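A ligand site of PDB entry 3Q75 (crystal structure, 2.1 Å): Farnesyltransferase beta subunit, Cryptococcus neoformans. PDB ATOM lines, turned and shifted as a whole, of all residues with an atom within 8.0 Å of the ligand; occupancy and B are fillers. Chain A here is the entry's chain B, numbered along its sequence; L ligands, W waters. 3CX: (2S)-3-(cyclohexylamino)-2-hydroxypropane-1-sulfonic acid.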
ATOM      1  N   LEU A  50      17.297  31.370 -36.834  1.00  0.00           N
ATOM      2  CA  LEU A  50      16.246  30.682 -36.078  1.00  0.00           C
ATOM      3  C   LEU A  50      15.772  29.436 -36.829  1.00  0.00           C
ATOM      4  O   LEU A  50      15.535  28.389 -36.223  1.00  0.00           O
ATOM      5  CB  LEU A  50      15.058  31.614 -35.824  1.00  0.00           C
ATOM      6  CG  LEU A  50      15.195  32.796 -34.852  1.00  0.00           C
ATOM      7  CD1 LEU A  50      14.153  33.857 -35.171  1.00  0.00           C
ATOM      8  CD2 LEU A  50      15.082  32.353 -33.401  1.00  0.00           C
ATOM      9  N   TYR A  58      24.391  21.012 -37.087  1.00  0.00           N
ATOM     10  CA  TYR A  58      24.212  22.004 -36.031  1.00  0.00           C
ATOM     11  C   TYR A  58      25.574  22.408 -35.449  1.00  0.00           C
ATOM     12  O   TYR A  58      26.390  21.540 -35.121  1.00  0.00           O
ATOM     13  CB  TYR A  58      23.254  21.499 -34.945  1.00  0.00           C
ATOM     14  CG  TYR A  58      22.990  22.521 -33.861  1.00  0.00           C
ATOM     15  CD1 TYR A  58      23.268  22.228 -32.525  1.00  0.00           C
ATOM     16  CD2 TYR A  58      22.483  23.781 -34.165  1.00  0.00           C
ATOM     17  CE1 TYR A  58      23.036  23.168 -31.520  1.00  0.00           C
ATOM     18  CE2 TYR A  58      22.252  24.735 -33.176  1.00  0.00           C
ATOM     19  CZ  TYR A  58      22.527  24.422 -31.861  1.00  0.00           C
ATOM     20  OH  TYR A  58      22.297  25.356 -30.881  1.00  0.00           O
ATOM     21  N   GLY A  60      26.239  24.171 -32.650  1.00  0.00           N
ATOM     22  CA  GLY A  60      26.271  24.366 -31.199  1.00  0.00           C
ATOM     23  C   GLY A  60      27.511  23.769 -30.551  1.00  0.00           C
ATOM     24  O   GLY A  60      27.966  22.685 -30.938  1.00  0.00           O
ATOM     25  N   LEU A  61      28.072  24.490 -29.578  1.00  0.00           N
ATOM     26  CA  LEU A  61      29.282  24.036 -28.886  1.00  0.00           C
ATOM     27  C   LEU A  61      28.999  22.723 -28.158  1.00  0.00           C
ATOM     28  O   LEU A  61      28.154  22.651 -27.273  1.00  0.00           O
ATOM     29  CB  LEU A  61      29.794  25.117 -27.913  1.00  0.00           C
ATOM     30  CG  LEU A  61      31.140  24.877 -27.216  1.00  0.00           C
ATOM     31  CD1 LEU A  61      32.300  24.775 -28.203  1.00  0.00           C
ATOM     32  CD2 LEU A  61      31.404  25.968 -26.187  1.00  0.00           C
ATOM     33  N   ILE A 486      27.129  36.344 -27.678  1.00  0.00           N
ATOM     34  CA  ILE A 486      27.140  34.879 -27.719  1.00  0.00           C
ATOM     35  C   ILE A 486      26.472  34.369 -28.993  1.00  0.00           C
ATOM     36  O   ILE A 486      25.240  34.211 -29.040  1.00  0.00           O
ATOM     37  CB  ILE A 486      26.478  34.238 -26.468  1.00  0.00           C
ATOM     38  CG1 ILE A 486      26.903  34.944 -25.169  1.00  0.00           C
ATOM     39  CG2 ILE A 486      26.780  32.741 -26.422  1.00  0.00           C
ATOM     40  CD1 ILE A 486      28.388  34.839 -24.850  1.00  0.00           C
ATOM     41  N   VAL A 487      27.291  34.130 -30.000  1.00  0.00           N
ATOM     42  CA  VAL A 487      26.827  33.596 -31.282  1.00  0.00           C
ATOM     43  C   VAL A 487      26.209  32.222 -31.087  1.00  0.00           C
ATOM     44  O   VAL A 487      26.795  31.345 -30.439  1.00  0.00           O
ATOM     45  CB  VAL A 487      27.988  33.541 -32.316  1.00  0.00           C
ATOM     46  CG1 VAL A 487      27.616  32.712 -33.540  1.00  0.00           C
ATOM     47  CG2 VAL A 487      28.433  34.945 -32.716  1.00  0.00           C
ATOM     48  N   GLY A 488      25.005  32.049 -31.628  1.00  0.00           N
ATOM     49  CA  GLY A 488      24.310  30.762 -31.611  1.00  0.00           C
ATOM     50  C   GLY A 488      23.392  30.530 -30.422  1.00  0.00           C
ATOM     51  O   GLY A 488      22.724  29.501 -30.341  1.00  0.00           O
ATOM     52  N   GLY A 489      23.359  31.485 -29.493  1.00  0.00           N
ATOM     53  CA  GLY A 489      22.503  31.370 -28.319  1.00  0.00           C
ATOM     54  C   GLY A 489      23.277  31.083 -27.052  1.00  0.00           C
ATOM     55  O   GLY A 489      24.421  30.615 -27.098  1.00  0.00           O
ATOM     56  N   LYS A 490      22.648  31.330 -25.909  1.00  0.00           N
ATOM     57  CA  LYS A 490      23.334  31.348 -24.609  1.00  0.00           C
ATOM     58  C   LYS A 490      23.930  30.020 -24.163  1.00  0.00           C
ATOM     59  O   LYS A 490      24.802  29.992 -23.292  1.00  0.00           O
ATOM     60  CB  LYS A 490      22.420  31.939 -23.529  1.00  0.00           C
ATOM     61  CG  LYS A 490      22.129  33.426 -23.740  1.00  0.00           C
ATOM     62  CD  LYS A 490      21.385  34.030 -22.570  1.00  0.00           C
ATOM     63  CE  LYS A 490      20.995  35.476 -22.853  1.00  0.00           C
ATOM     64  NZ  LYS A 490      20.139  36.043 -21.758  1.00  0.00           N
ATOM     65  N   ASP A 491      23.482  28.917 -24.763  1.00  0.00           N
ATOM     66  CA  ASP A 491      24.063  27.596 -24.480  1.00  0.00           C
ATOM     67  C   ASP A 491      25.499  27.452 -25.005  1.00  0.00           C
ATOM     68  O   ASP A 491      26.230  26.558 -24.579  1.00  0.00           O
ATOM     69  CB  ASP A 491      23.168  26.479 -25.038  1.00  0.00           C
ATOM     70  CG  ASP A 491      21.937  26.229 -24.170  1.00  0.00           C
ATOM     71  OD1 ASP A 491      22.007  26.359 -22.931  1.00  0.00           O
ATOM     72  OD2 ASP A 491      20.875  25.895 -24.741  1.00  0.00           O
ATOM     73  N   ASN A 492      25.898  28.338 -25.934  1.00  0.00           N
ATOM     74  CA  ASN A 492      27.276  28.382 -26.426  1.00  0.00           C
ATOM     75  C   ASN A 492      28.231  29.172 -25.513  1.00  0.00           C
ATOM     76  O   ASN A 492      29.455  29.101 -25.676  1.00  0.00           O
ATOM     77  CB  ASN A 492      27.337  28.963 -27.838  1.00  0.00           C
ATOM     78  CG  ASN A 492      26.760  28.017 -28.880  1.00  0.00           C
ATOM     79  OD1 ASN A 492      26.692  26.809 -28.684  1.00  0.00           O
ATOM     80  ND2 ASN A 492      26.353  28.586 -30.005  1.00  0.00           N
ATOM     81  N   ARG A 493      27.663  29.919 -24.576  1.00  0.00           N
ATOM     82  CA  ARG A 493      28.445  30.739 -23.653  1.00  0.00           C
ATOM     83  C   ARG A 493      29.443  29.922 -22.843  1.00  0.00           C
ATOM     84  O   ARG A 493      29.101  28.900 -22.231  1.00  0.00           O
ATOM     85  CB  ARG A 493      27.534  31.506 -22.696  1.00  0.00           C
ATOM     86  CG  ARG A 493      28.191  32.722 -22.058  1.00  0.00           C
ATOM     87  CD  ARG A 493      27.504  33.106 -20.758  1.00  0.00           C
ATOM     88  NE  ARG A 493      28.178  32.454 -19.635  1.00  0.00           N
ATOM     89  CZ  ARG A 493      29.066  33.039 -18.847  1.00  0.00           C
ATOM     90  NH1 ARG A 493      29.390  34.312 -19.007  1.00  0.00           N
ATOM     91  NH2 ARG A 493      29.613  32.337 -17.868  1.00  0.00           N
HETATM   92  OAA 3CX L   1      17.633  32.547 -25.847  1.00  0.00           O
HETATM   93  OAB 3CX L   1      19.019  31.357 -24.227  1.00  0.00           O
HETATM   94  OAC 3CX L   1      20.382  29.082 -25.553  1.00  0.00           O
HETATM   95  OAD 3CX L   1      19.939  32.102 -26.302  1.00  0.00           O
HETATM   96  CAE 3CX L   1      19.132  22.559 -27.889  1.00  0.00           C
HETATM   97  CAF 3CX L   1      17.934  23.494 -27.708  1.00  0.00           C
HETATM   98  CAG 3CX L   1      20.238  23.249 -28.699  1.00  0.00           C
HETATM   99  CAH 3CX L   1      18.355  24.828 -27.053  1.00  0.00           C
HETATM  100  CAI 3CX L   1      20.690  24.552 -28.017  1.00  0.00           C
HETATM  101  CAJ 3CX L   1      19.218  27.859 -27.328  1.00  0.00           C
HETATM  102  CAK 3CX L   1      18.321  30.015 -26.529  1.00  0.00           C
HETATM  103  NAL 3CX L   1      20.000  26.664 -27.019  1.00  0.00           N
HETATM  104  CAM 3CX L   1      19.089  28.766 -26.105  1.00  0.00           C
HETATM  105  CAN 3CX L   1      19.519  25.521 -27.803  1.00  0.00           C
HETATM  106  SAO 3CX L   1      18.762  31.582 -25.684  1.00  0.00           S
HETATM  107  O   HOH W   1      19.280  29.894 -29.885  1.00  0.00           O
HETATM  108  O   HOH W   2      22.425  27.880 -28.216  1.00  0.00           O
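An oxygen (OAC) of the ligand is in hydrogen-bond range of the backbone NH (N) of Asp 491 (3.2 Å). OD2 of Asp 491 is in salt-bridge range of NAL of the ligand (2.6 Å). N of Lys 490 sits at hydrogen-bond distance from OAD of the ligand (2.8 Å).
Water W2 lies within hydrogen-bond range of the backbone carbonyl oxygen of Gly 488 (2.7 Å) and a nitrogen (NAL) of the ligand (3.0 Å).
Residues that only touch the ligand: Gly 489 (3.3 Å) and Tyr 58 (3.4 Å). Four residues have an atom within 4 Å of the ligand: Tyr 58, Gly 489, Lys 490 and Asp 491. The nearest printed residue that does not touch the ligand is Gly 488 (4.9 Å).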
